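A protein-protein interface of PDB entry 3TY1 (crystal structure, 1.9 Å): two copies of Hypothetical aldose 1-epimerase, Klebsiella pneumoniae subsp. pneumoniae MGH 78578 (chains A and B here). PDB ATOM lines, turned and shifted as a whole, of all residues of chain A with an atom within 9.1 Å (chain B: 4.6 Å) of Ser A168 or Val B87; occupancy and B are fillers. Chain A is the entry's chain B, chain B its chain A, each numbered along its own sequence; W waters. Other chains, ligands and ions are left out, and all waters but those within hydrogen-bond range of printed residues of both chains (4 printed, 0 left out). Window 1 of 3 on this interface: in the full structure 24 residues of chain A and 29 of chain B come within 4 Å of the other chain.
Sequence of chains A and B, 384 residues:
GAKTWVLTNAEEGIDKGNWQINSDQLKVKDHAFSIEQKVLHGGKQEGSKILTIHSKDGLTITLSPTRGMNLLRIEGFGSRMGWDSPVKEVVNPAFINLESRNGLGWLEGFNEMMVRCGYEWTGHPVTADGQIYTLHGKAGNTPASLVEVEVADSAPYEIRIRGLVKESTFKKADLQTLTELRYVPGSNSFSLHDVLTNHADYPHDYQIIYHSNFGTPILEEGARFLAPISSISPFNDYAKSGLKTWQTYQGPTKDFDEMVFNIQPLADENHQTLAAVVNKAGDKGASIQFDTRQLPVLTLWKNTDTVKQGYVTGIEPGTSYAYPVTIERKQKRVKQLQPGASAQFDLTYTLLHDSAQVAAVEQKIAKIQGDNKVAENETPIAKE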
ATOM      1  N   GLU A 120       1.093 -20.186 -31.738  1.00  0.00           N
ATOM      2  CA  GLU A 120       2.030 -19.178 -32.231  1.00  0.00           C
ATOM      3  C   GLU A 120       2.160 -19.252 -33.764  1.00  0.00           C
ATOM      4  O   GLU A 120       2.348 -18.205 -34.441  1.00  0.00           O
ATOM      5  CB  GLU A 120       3.399 -19.316 -31.520  1.00  0.00           C
ATOM      6  CG  GLU A 120       4.345 -18.214 -31.787  1.00  0.00           C
ATOM      7  CD  GLU A 120       5.717 -18.451 -31.160  1.00  0.00           C
ATOM      8  OE1 GLU A 120       5.803 -19.199 -30.166  1.00  0.00           O
ATOM      9  OE2 GLU A 120       6.719 -17.836 -31.630  1.00  0.00           O
ATOM     10  N   LYS A 138       3.271 -25.765 -31.769  1.00  0.00           N
ATOM     11  CA  LYS A 138       3.784 -26.330 -30.544  1.00  0.00           C
ATOM     12  C   LYS A 138       2.742 -26.743 -29.536  1.00  0.00           C
ATOM     13  O   LYS A 138       3.086 -27.514 -28.608  1.00  0.00           O
ATOM     14  CB  LYS A 138       4.792 -25.326 -29.902  1.00  0.00           C
ATOM     15  CG  LYS A 138       6.125 -25.282 -30.659  1.00  0.00           C
ATOM     16  CD  LYS A 138       7.325 -24.707 -29.895  1.00  0.00           C
ATOM     17  CE  LYS A 138       7.815 -25.546 -28.723  1.00  0.00           C
ATOM     18  NZ  LYS A 138       8.742 -24.730 -27.854  1.00  0.00           N
ATOM     19  N   THR A 142       3.034 -29.614 -26.055  1.00  0.00           N
ATOM     20  CA  THR A 142       3.354 -28.864 -24.854  1.00  0.00           C
ATOM     21  C   THR A 142       2.580 -29.462 -23.678  1.00  0.00           C
ATOM     22  O   THR A 142       1.327 -29.491 -23.703  1.00  0.00           O
ATOM     23  CB  THR A 142       3.017 -27.387 -25.017  1.00  0.00           C
ATOM     24  OG1 THR A 142       3.781 -26.842 -26.104  1.00  0.00           O
ATOM     25  CG2 THR A 142       3.403 -26.535 -23.703  1.00  0.00           C
ATOM     26  N   SER A 145       0.300 -26.838 -17.991  1.00  0.00           N
ATOM     27  CA  SER A 145       0.807 -26.267 -16.768  1.00  0.00           C
ATOM     28  C   SER A 145      -0.202 -26.291 -15.602  1.00  0.00           C
ATOM     29  O   SER A 145       0.196 -26.247 -14.442  1.00  0.00           O
ATOM     30  CB  SER A 145       1.196 -24.788 -17.010  1.00  0.00           C
ATOM     31  OG  SER A 145       2.179 -24.648 -18.035  1.00  0.00           O
ATOM     32  N   LEU A 164      -4.244 -25.502 -19.112  1.00  0.00           N
ATOM     33  CA  LEU A 164      -3.567 -24.295 -19.567  1.00  0.00           C
ATOM     34  C   LEU A 164      -2.318 -24.722 -20.278  1.00  0.00           C
ATOM     35  O   LEU A 164      -1.454 -25.360 -19.662  1.00  0.00           O
ATOM     36  CB  LEU A 164      -3.232 -23.362 -18.379  1.00  0.00           C
ATOM     37  CG  LEU A 164      -2.607 -22.026 -18.722  1.00  0.00           C
ATOM     38  CD1 LEU A 164      -3.566 -21.119 -19.493  1.00  0.00           C
ATOM     39  CD2 LEU A 164      -2.057 -21.398 -17.395  1.00  0.00           C
ATOM     40  N   VAL A 165      -2.216 -24.375 -21.569  1.00  0.00           N
ATOM     41  CA  VAL A 165      -1.059 -24.737 -22.403  1.00  0.00           C
ATOM     42  C   VAL A 165      -0.330 -23.448 -22.784  1.00  0.00           C
ATOM     43  O   VAL A 165      -0.869 -22.609 -23.484  1.00  0.00           O
ATOM     44  CB  VAL A 165      -1.533 -25.498 -23.657  1.00  0.00           C
ATOM     45  CG1 VAL A 165      -0.387 -25.961 -24.569  1.00  0.00           C
ATOM     46  CG2 VAL A 165      -2.384 -26.715 -23.204  1.00  0.00           C
ATOM     47  N   LYS A 166       0.932 -23.325 -22.352  1.00  0.00           N
ATOM     48  CA  LYS A 166       1.653 -22.084 -22.470  1.00  0.00           C
ATOM     49  C   LYS A 166       2.675 -22.117 -23.602  1.00  0.00           C
ATOM     50  O   LYS A 166       3.359 -23.154 -23.808  1.00  0.00           O
ATOM     51  CB  LYS A 166       2.383 -21.807 -21.164  1.00  0.00           C
ATOM     52  CG  LYS A 166       1.449 -21.619 -19.982  1.00  0.00           C
ATOM     53  CD  LYS A 166       2.345 -21.116 -18.771  1.00  0.00           C
ATOM     54  CE  LYS A 166       1.581 -20.751 -17.552  1.00  0.00           C
ATOM     55  NZ  LYS A 166       2.512 -19.932 -16.714  1.00  0.00           N
ATOM     56  N   GLU A 167       2.748 -20.991 -24.320  1.00  0.00           N
ATOM     57  CA  GLU A 167       3.760 -20.724 -25.350  1.00  0.00           C
ATOM     58  C   GLU A 167       4.429 -19.403 -24.989  1.00  0.00           C
ATOM     59  O   GLU A 167       4.203 -18.369 -25.643  1.00  0.00           O
ATOM     60  CB  GLU A 167       3.133 -20.662 -26.735  1.00  0.00           C
ATOM     61  CG  GLU A 167       2.523 -21.996 -27.123  1.00  0.00           C
ATOM     62  CD  GLU A 167       1.789 -22.004 -28.482  1.00  0.00           C
ATOM     63  OE1 GLU A 167       2.466 -21.863 -29.544  1.00  0.00           O
ATOM     64  OE2 GLU A 167       0.541 -22.233 -28.470  1.00  0.00           O
ATOM     65  N   SER A 168       5.285 -19.492 -23.963  1.00  0.00           N
ATOM     66  CA  SER A 168       5.927 -18.381 -23.326  1.00  0.00           C
ATOM     67  C   SER A 168       7.408 -18.436 -23.627  1.00  0.00           C
ATOM     68  O   SER A 168       8.097 -19.420 -23.290  1.00  0.00           O
ATOM     69  CB  SER A 168       5.743 -18.465 -21.804  1.00  0.00           C
ATOM     70  OG  SER A 168       4.388 -18.462 -21.447  1.00  0.00           O
ATOM     71  N   THR A 169       7.909 -17.371 -24.260  1.00  0.00           N
ATOM     72  CA  THR A 169       9.328 -17.293 -24.650  1.00  0.00           C
ATOM     73  C   THR A 169       9.838 -15.869 -24.478  1.00  0.00           C
ATOM     74  O   THR A 169       9.246 -14.942 -25.038  1.00  0.00           O
ATOM     75  CB  THR A 169       9.481 -17.728 -26.138  1.00  0.00           C
ATOM     76  OG1 THR A 169       8.923 -19.022 -26.337  1.00  0.00           O
ATOM     77  CG2 THR A 169      10.946 -17.720 -26.621  1.00  0.00           C
ATOM     78  N   PHE A 170      10.974 -15.694 -23.786  1.00  0.00           N
ATOM     79  CA  PHE A 170      11.509 -14.363 -23.539  1.00  0.00           C
ATOM     80  C   PHE A 170      11.842 -13.733 -24.893  1.00  0.00           C
ATOM     81  O   PHE A 170      12.393 -14.398 -25.772  1.00  0.00           O
ATOM     82  CB  PHE A 170      12.744 -14.415 -22.650  1.00  0.00           C
ATOM     83  CG  PHE A 170      13.377 -13.086 -22.373  1.00  0.00           C
ATOM     84  CD1 PHE A 170      12.640 -12.047 -21.809  1.00  0.00           C
ATOM     85  CD2 PHE A 170      14.731 -12.878 -22.652  1.00  0.00           C
ATOM     86  CE1 PHE A 170      13.232 -10.815 -21.575  1.00  0.00           C
ATOM     87  CE2 PHE A 170      15.332 -11.646 -22.394  1.00  0.00           C
ATOM     88  CZ  PHE A 170      14.595 -10.633 -21.844  1.00  0.00           C
ATOM     89  N   LYS A 171      11.430 -12.481 -25.044  1.00  0.00           N
ATOM     90  CA  LYS A 171      11.631 -11.666 -26.262  1.00  0.00           C
ATOM     91  C   LYS A 171      10.773 -12.037 -27.453  1.00  0.00           C
ATOM     92  O   LYS A 171      10.784 -11.311 -28.442  1.00  0.00           O
ATOM     93  CB  LYS A 171      13.127 -11.547 -26.649  1.00  0.00           C
ATOM     94  CG  LYS A 171      13.813 -10.539 -25.717  1.00  0.00           C
ATOM     95  CD  LYS A 171      15.230 -10.280 -26.029  1.00  0.00           C
ATOM     96  CE  LYS A 171      15.781  -9.217 -25.109  1.00  0.00           C
ATOM     97  NZ  LYS A 171      15.628  -7.799 -25.525  1.00  0.00           N
ATOM     98  N   LYS A 172       9.956 -13.082 -27.362  1.00  0.00           N
ATOM     99  CA  LYS A 172       9.223 -13.554 -28.544  1.00  0.00           C
ATOM    100  C   LYS A 172       7.711 -13.523 -28.389  1.00  0.00           C
ATOM    101  O   LYS A 172       7.026 -12.964 -29.229  1.00  0.00           O
ATOM    102  CB  LYS A 172       9.640 -14.973 -28.899  1.00  0.00           C
ATOM    103  CG  LYS A 172      11.133 -15.145 -29.298  1.00  0.00           C
ATOM    104  CD  LYS A 172      11.443 -14.495 -30.596  1.00  0.00           C
ATOM    105  CE  LYS A 172      12.809 -14.918 -31.119  1.00  0.00           C
ATOM    106  NZ  LYS A 172      12.885 -14.683 -32.585  1.00  0.00           N
ATOM    107  N   ALA A 173       7.175 -14.166 -27.359  1.00  0.00           N
ATOM    108  CA  ALA A 173       5.691 -14.283 -27.215  1.00  0.00           C
ATOM    109  C   ALA A 173       5.329 -14.753 -25.832  1.00  0.00           C
ATOM    110  O   ALA A 173       6.177 -15.297 -25.095  1.00  0.00           O
ATOM    111  CB  ALA A 173       5.107 -15.264 -28.195  1.00  0.00           C
ATOM    112  N   ASP A 174       4.098 -14.450 -25.451  1.00  0.00           N
ATOM    113  CA  ASP A 174       3.538 -15.043 -24.267  1.00  0.00           C
ATOM    114  C   ASP A 174       2.079 -15.301 -24.550  1.00  0.00           C
ATOM    115  O   ASP A 174       1.209 -14.554 -24.106  1.00  0.00           O
ATOM    116  CB  ASP A 174       3.723 -14.186 -23.031  1.00  0.00           C
ATOM    117  CG  ASP A 174       3.417 -14.977 -21.707  1.00  0.00           C
ATOM    118  OD1 ASP A 174       3.079 -16.218 -21.777  1.00  0.00           O
ATOM    119  OD2 ASP A 174       3.459 -14.306 -20.632  1.00  0.00           O
ATOM    120  N   LEU A 175       1.867 -16.343 -25.347  1.00  0.00           N
ATOM    121  CA  LEU A 175       0.553 -16.859 -25.696  1.00  0.00           C
ATOM    122  C   LEU A 175       0.258 -18.061 -24.811  1.00  0.00           C
ATOM    123  O   LEU A 175       1.111 -18.908 -24.613  1.00  0.00           O
ATOM    124  CB  LEU A 175       0.460 -17.275 -27.164  1.00  0.00           C
ATOM    125  CG  LEU A 175       0.602 -16.155 -28.203  1.00  0.00           C
ATOM    126  CD1 LEU A 175       0.675 -16.789 -29.602  1.00  0.00           C
ATOM    127  CD2 LEU A 175      -0.577 -15.149 -28.112  1.00  0.00           C
ATOM    128  N   GLN A 176      -0.940 -18.084 -24.236  1.00  0.00           N
ATOM    129  CA  GLN A 176      -1.343 -19.157 -23.359  1.00  0.00           C
ATOM    130  C   GLN A 176      -2.788 -19.450 -23.655  1.00  0.00           C
ATOM    131  O   GLN A 176      -3.604 -18.513 -23.714  1.00  0.00           O
ATOM    132  CB  GLN A 176      -1.212 -18.723 -21.893  1.00  0.00           C
ATOM    133  CG  GLN A 176       0.198 -18.289 -21.481  1.00  0.00           C
ATOM    134  CD  GLN A 176       0.298 -17.933 -20.010  1.00  0.00           C
ATOM    135  OE1 GLN A 176      -0.511 -18.383 -19.210  1.00  0.00           O
ATOM    136  NE2 GLN A 176       1.319 -17.121 -19.648  1.00  0.00           N
ATOM    137  N   THR A 177      -3.094 -20.737 -23.797  1.00  0.00           N
ATOM    138  CA  THR A 177      -4.436 -21.184 -24.076  1.00  0.00           C
ATOM    139  C   THR A 177      -5.033 -21.973 -22.935  1.00  0.00           C
ATOM    140  O   THR A 177      -4.484 -23.000 -22.542  1.00  0.00           O
ATOM    141  CB  THR A 177      -4.484 -22.022 -25.318  1.00  0.00           C
ATOM    142  OG1 THR A 177      -3.982 -21.231 -26.374  1.00  0.00           O
ATOM    143  CG2 THR A 177      -5.991 -22.389 -25.668  1.00  0.00           C
ATOM    144  N   THR A 197      -5.051 -16.314 -24.813  1.00  0.00           N
ATOM    145  CA  THR A 197      -4.803 -14.967 -24.288  1.00  0.00           C
ATOM    146  C   THR A 197      -3.378 -14.568 -24.638  1.00  0.00           C
ATOM    147  O   THR A 197      -2.449 -15.397 -24.535  1.00  0.00           O
ATOM    148  CB  THR A 197      -5.034 -14.895 -22.746  1.00  0.00           C
ATOM    149  OG1 THR A 197      -6.409 -15.179 -22.476  1.00  0.00           O
ATOM    150  CG2 THR A 197      -4.742 -13.497 -22.164  1.00  0.00           C
ATOM    151  N   HIS A 199      -0.721 -12.666 -23.196  1.00  0.00           N
ATOM    152  CA  HIS A 199      -0.242 -12.092 -21.911  1.00  0.00           C
ATOM    153  C   HIS A 199       0.897 -11.051 -22.032  1.00  0.00           C
ATOM    154  O   HIS A 199       1.318 -10.497 -21.016  1.00  0.00           O
ATOM    155  CB  HIS A 199       0.252 -13.224 -21.023  1.00  0.00           C
ATOM    156  CG  HIS A 199      -0.839 -14.117 -20.540  1.00  0.00           C
ATOM    157  ND1 HIS A 199      -1.375 -14.003 -19.282  1.00  0.00           N
ATOM    158  CD2 HIS A 199      -1.519 -15.123 -21.155  1.00  0.00           C
ATOM    159  CE1 HIS A 199      -2.356 -14.881 -19.140  1.00  0.00           C
ATOM    160  NE2 HIS A 199      -2.464 -15.574 -20.257  1.00  0.00           N
ATOM    161  N   ALA A 200       1.429 -10.849 -23.234  1.00  0.00           N
ATOM    162  CA  ALA A 200       2.487  -9.845 -23.491  1.00  0.00           C
ATOM    163  C   ALA A 200       1.908  -8.439 -23.606  1.00  0.00           C
ATOM    164  O   ALA A 200       0.695  -8.253 -23.721  1.00  0.00           O
ATOM    165  CB  ALA A 200       3.226 -10.203 -24.796  1.00  0.00           C
ATOM    166  N   SER B  85      10.487 -12.763 -15.542  1.00  0.00           N
ATOM    167  CA  SER B  85      10.468 -13.152 -16.948  1.00  0.00           C
ATOM    168  C   SER B  85       9.081 -13.654 -17.325  1.00  0.00           C
ATOM    169  O   SER B  85       8.341 -14.138 -16.449  1.00  0.00           O
ATOM    170  CB  SER B  85      11.479 -14.250 -17.131  1.00  0.00           C
ATOM    171  OG  SER B  85      11.455 -14.847 -18.397  1.00  0.00           O
ATOM    172  N   PRO B  86       8.714 -13.577 -18.629  1.00  0.00           N
ATOM    173  CA  PRO B  86       7.515 -14.290 -19.048  1.00  0.00           C
ATOM    174  C   PRO B  86       7.575 -15.807 -18.853  1.00  0.00           C
ATOM    175  O   PRO B  86       6.531 -16.444 -18.849  1.00  0.00           O
ATOM    176  CB  PRO B  86       7.414 -13.952 -20.548  1.00  0.00           C
ATOM    177  CG  PRO B  86       8.842 -13.586 -20.973  1.00  0.00           C
ATOM    178  CD  PRO B  86       9.329 -12.841 -19.761  1.00  0.00           C
ATOM    179  N   VAL B  87       8.770 -16.387 -18.797  1.00  0.00           N
ATOM    180  CA  VAL B  87       8.979 -17.822 -18.575  1.00  0.00           C
ATOM    181  C   VAL B  87       8.923 -18.009 -17.024  1.00  0.00           C
ATOM    182  O   VAL B  87       9.856 -17.627 -16.291  1.00  0.00           O
ATOM    183  CB  VAL B  87      10.337 -18.305 -19.115  1.00  0.00           C
ATOM    184  CG1 VAL B  87      10.551 -19.803 -18.792  1.00  0.00           C
ATOM    185  CG2 VAL B  87      10.475 -18.026 -20.625  1.00  0.00           C
ATOM    186  N   LYS B  88       7.812 -18.528 -16.540  1.00  0.00           N
ATOM    187  CA  LYS B  88       7.572 -18.679 -15.111  1.00  0.00           C
ATOM    188  C   LYS B  88       8.004 -20.052 -14.592  1.00  0.00           C
ATOM    189  O   LYS B  88       8.264 -20.211 -13.417  1.00  0.00           O
ATOM    190  CB  LYS B  88       6.100 -18.486 -14.791  1.00  0.00           C
ATOM    191  CG  LYS B  88       5.497 -17.185 -15.260  1.00  0.00           C
ATOM    192  CD  LYS B  88       6.009 -15.988 -14.550  1.00  0.00           C
ATOM    193  CE  LYS B  88       5.315 -14.682 -15.055  1.00  0.00           C
ATOM    194  NZ  LYS B  88       6.236 -13.469 -14.803  1.00  0.00           N
ATOM    195  N   GLU B  89       8.125 -21.024 -15.461  1.00  0.00           N
ATOM    196  CA  GLU B  89       8.497 -22.378 -15.055  1.00  0.00           C
ATOM    197  C   GLU B  89      10.028 -22.552 -15.013  1.00  0.00           C
ATOM    198  O   GLU B  89      10.736 -21.852 -15.719  1.00  0.00           O
ATOM    199  CB  GLU B  89       7.883 -23.345 -16.075  1.00  0.00           C
ATOM    200  CG  GLU B  89       6.328 -23.371 -15.821  1.00  0.00           C
ATOM    201  CD  GLU B  89       5.528 -24.206 -16.801  1.00  0.00           C
ATOM    202  OE1 GLU B  89       6.116 -24.879 -17.699  1.00  0.00           O
ATOM    203  OE2 GLU B  89       4.284 -24.137 -16.662  1.00  0.00           O
ATOM    204  N   VAL B  91      12.228 -24.728 -16.400  1.00  0.00           N
ATOM    205  CA  VAL B  91      12.070 -25.626 -17.538  1.00  0.00           C
ATOM    206  C   VAL B  91      13.107 -26.735 -17.502  1.00  0.00           C
ATOM    207  O   VAL B  91      14.334 -26.477 -17.439  1.00  0.00           O
ATOM    208  CB  VAL B  91      12.075 -24.873 -18.866  1.00  0.00           C
ATOM    209  CG1 VAL B  91      11.934 -25.828 -20.069  1.00  0.00           C
ATOM    210  CG2 VAL B  91      10.983 -23.757 -18.849  1.00  0.00           C
ATOM    211  N   LEU B 107      15.980 -19.048 -25.100  1.00  0.00           N
ATOM    212  CA  LEU B 107      14.994 -18.064 -24.678  1.00  0.00           C
ATOM    213  C   LEU B 107      13.734 -18.667 -24.014  1.00  0.00           C
ATOM    214  O   LEU B 107      13.047 -17.987 -23.262  1.00  0.00           O
ATOM    215  CB  LEU B 107      14.613 -17.155 -25.838  1.00  0.00           C
ATOM    216  CG  LEU B 107      15.680 -16.200 -26.427  1.00  0.00           C
ATOM    217  CD1 LEU B 107      15.065 -15.517 -27.648  1.00  0.00           C
ATOM    218  CD2 LEU B 107      16.164 -15.168 -25.418  1.00  0.00           C
ATOM    219  N   GLU B 108      13.433 -19.928 -24.303  1.00  0.00           N
ATOM    220  CA  GLU B 108      12.276 -20.616 -23.741  1.00  0.00           C
ATOM    221  C   GLU B 108      12.456 -20.985 -22.271  1.00  0.00           C
ATOM    222  O   GLU B 108      11.468 -21.335 -21.595  1.00  0.00           O
ATOM    223  CB  GLU B 108      11.919 -21.856 -24.593  1.00  0.00           C
ATOM    224  CG  GLU B 108      11.623 -21.476 -26.067  1.00  0.00           C
ATOM    225  CD  GLU B 108      11.162 -22.617 -26.961  1.00  0.00           C
ATOM    226  OE1 GLU B 108      11.149 -23.800 -26.540  1.00  0.00           O
ATOM    227  OE2 GLU B 108      10.780 -22.312 -28.116  1.00  0.00           O
ATOM    228  N   GLY B 109      13.695 -20.940 -21.784  1.00  0.00           N
ATOM    229  CA  GLY B 109      14.008 -21.245 -20.385  1.00  0.00           C
ATOM    230  C   GLY B 109      14.493 -20.101 -19.510  1.00  0.00           C
ATOM    231  O   GLY B 109      14.667 -20.274 -18.293  1.00  0.00           O
ATOM    232  N   PHE B 110      14.632 -18.917 -20.092  1.00  0.00           N
ATOM    233  CA  PHE B 110      15.357 -17.832 -19.414  1.00  0.00           C
ATOM    234  C   PHE B 110      14.539 -17.026 -18.445  1.00  0.00           C
ATOM    235  O   PHE B 110      13.644 -16.247 -18.836  1.00  0.00           O
ATOM    236  CB  PHE B 110      16.058 -16.915 -20.448  1.00  0.00           C
ATOM    237  CG  PHE B 110      16.881 -15.787 -19.834  1.00  0.00           C
ATOM    238  CD1 PHE B 110      17.691 -16.001 -18.738  1.00  0.00           C
ATOM    239  CD2 PHE B 110      16.923 -14.542 -20.435  1.00  0.00           C
ATOM    240  CE1 PHE B 110      18.488 -14.968 -18.193  1.00  0.00           C
ATOM    241  CE2 PHE B 110      17.699 -13.529 -19.906  1.00  0.00           C
ATOM    242  CZ  PHE B 110      18.482 -13.745 -18.788  1.00  0.00           C
ATOM    243  N   ASN B 111      14.816 -17.257 -17.152  1.00  0.00           N
ATOM    244  CA  ASN B 111      14.228 -16.464 -16.086  1.00  0.00           C
ATOM    245  C   ASN B 111      15.118 -16.241 -14.845  1.00  0.00           C
ATOM    246  O   ASN B 111      14.678 -15.670 -13.856  1.00  0.00           O
ATOM    247  CB  ASN B 111      12.906 -17.090 -15.686  1.00  0.00           C
ATOM    248  CG  ASN B 111      13.072 -18.494 -15.132  1.00  0.00           C
ATOM    249  OD1 ASN B 111      14.189 -18.908 -14.713  1.00  0.00           O
ATOM    250  ND2 ASN B 111      11.948 -19.209 -15.047  1.00  0.00           N
HETATM  251  O   HOH W   1       8.797 -21.652 -21.829  1.00  0.00           O
HETATM  252  O   HOH W   2       3.372 -22.185 -15.246  1.00  0.00           O
HETATM  253  O   HOH W   3      11.057 -23.884 -30.058  1.00  0.00           O
HETATM  254  O   HOH W   4       3.983 -15.444 -18.323  1.00  0.00           O
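The side-chain carboxylate (OE1) of Glu B108 lies within salt-bridge range of the side-chain amino group (NZ) of Lys A138 (2.9 Å).
The backbone carbonyl oxygen (O) of Leu B107 lies within hydrogen-bond range of the backbone NH (N) of Phe A170, at 3.1 Å.
The side-chain carboxylate (OE2) of Glu B89 is in hydrogen-bond range of the side-chain hydroxyl (OG) of Ser A145, at 2.6 Å.
ND2 of Asn B111 is in hydrogen-bond range of O of Glu B89.
O of Phe B110 is in hydrogen-bond range of OG of Ser B85 (2.6 Å).
The backbone carbonyl oxygen of Leu A164 is in hydrogen-bond range of the backbone NH of Ser A145 (2.8 Å).
The backbone carbonyl oxygen of Asp A174 lies within hydrogen-bond range of the backbone NH of His A199 (2.8 Å).
The side-chain hydroxyl (OG) of Ser B85 sits close to the backbone NH (N) of Val B87 (3.1 Å).
OG of Ser A168 lies within hydrogen-bond range of OD1 of Asp A174.
Of the printed residues of chain B, Phe A170 touches Pro B86 (3.8 Å), Val B87 (3.96 Å), Leu B107 (3.1 Å) and Phe B110 (3.5 Å).
Of the printed residues of chain B, Asp A174 touches Pro B86 (3.97 Å).
No residue of chain A comes within 4 Å of Ser B85.
Of chain A, only Ser A168 (3.8 Å) and Phe A170 (3.96 Å) come within 4 Å of Val B87.
Printed residues of chain A within 4 Å of Glu B89: Ser A145 (2.6 Å).
Printed residues of chain A within 4 Å of Glu B108: Lys A138 and Thr A169.
Of the printed residues of chain A, Phe B110 touches Phe A170.
The nearest residue of chain B that does not touch Ser A168 is Glu B108 (4.2 Å).
No position is printed for both chains.
Of the 11 pairs that touch across the chains among the printed residues, none has its exchanged pair printed and touching as well.
Of the 21 printed residues of chain A, 6 touch a printed residue of chain B.
Printed residues of chain A that touch a printed residue of chain B: Lys A138, Ser A145, Ser A168, Thr A169, Phe A170 and Asp A174.
Hydrophobic or aromatic side chains of chain A that line the printed part of chain B: Phe A170.
Of the 11 printed residues of chain B, 6 touch a printed residue of chain A.
Along chain B the printed residues that touch a printed residue of chain A span positions 86 to 110.
Among the printed residues, Asp or Glu carboxylates within 4 Å of a Lys or Arg side-chain nitrogen of the other chain: Lys A138 with Glu B108 (2.9 Å).
Ser A168 touches Pro B86 (CB to O, 3.7 Å).
Ser A168 touches Val B87.
Leu B107 touches Thr A169.
Thr A169 touches Glu B108 (OG1 to CG, 3.7 Å).
Phe A170 touches Pro B86.
Val B87 touches Phe A170.
Phe A170 touches Phe B110.
Pro B86 touches Asp A174.
Water W3 bridges the side-chain carboxylate of Glu B108 (2.5 Å) and the side-chain amino group of Lys A138 (3.3 Å).
Water W2 bridges the side-chain carboxylate (OE2) of Glu B89 (2.6 Å) and the side-chain amino group (NZ) of Lys A166 (2.8 Å).
Water W4 lies within hydrogen-bond range of the side-chain carboxylate of Asp A174, the backbone carbonyl oxygen of Pro B86 and the side-chain amide nitrogen of Gln A176.
Water W1 lies within hydrogen-bond range of the backbone carbonyl oxygen (O) of Glu B108 (2.7 Å) and the backbone carbonyl oxygen (O) of Ser A168 (2.8 Å).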
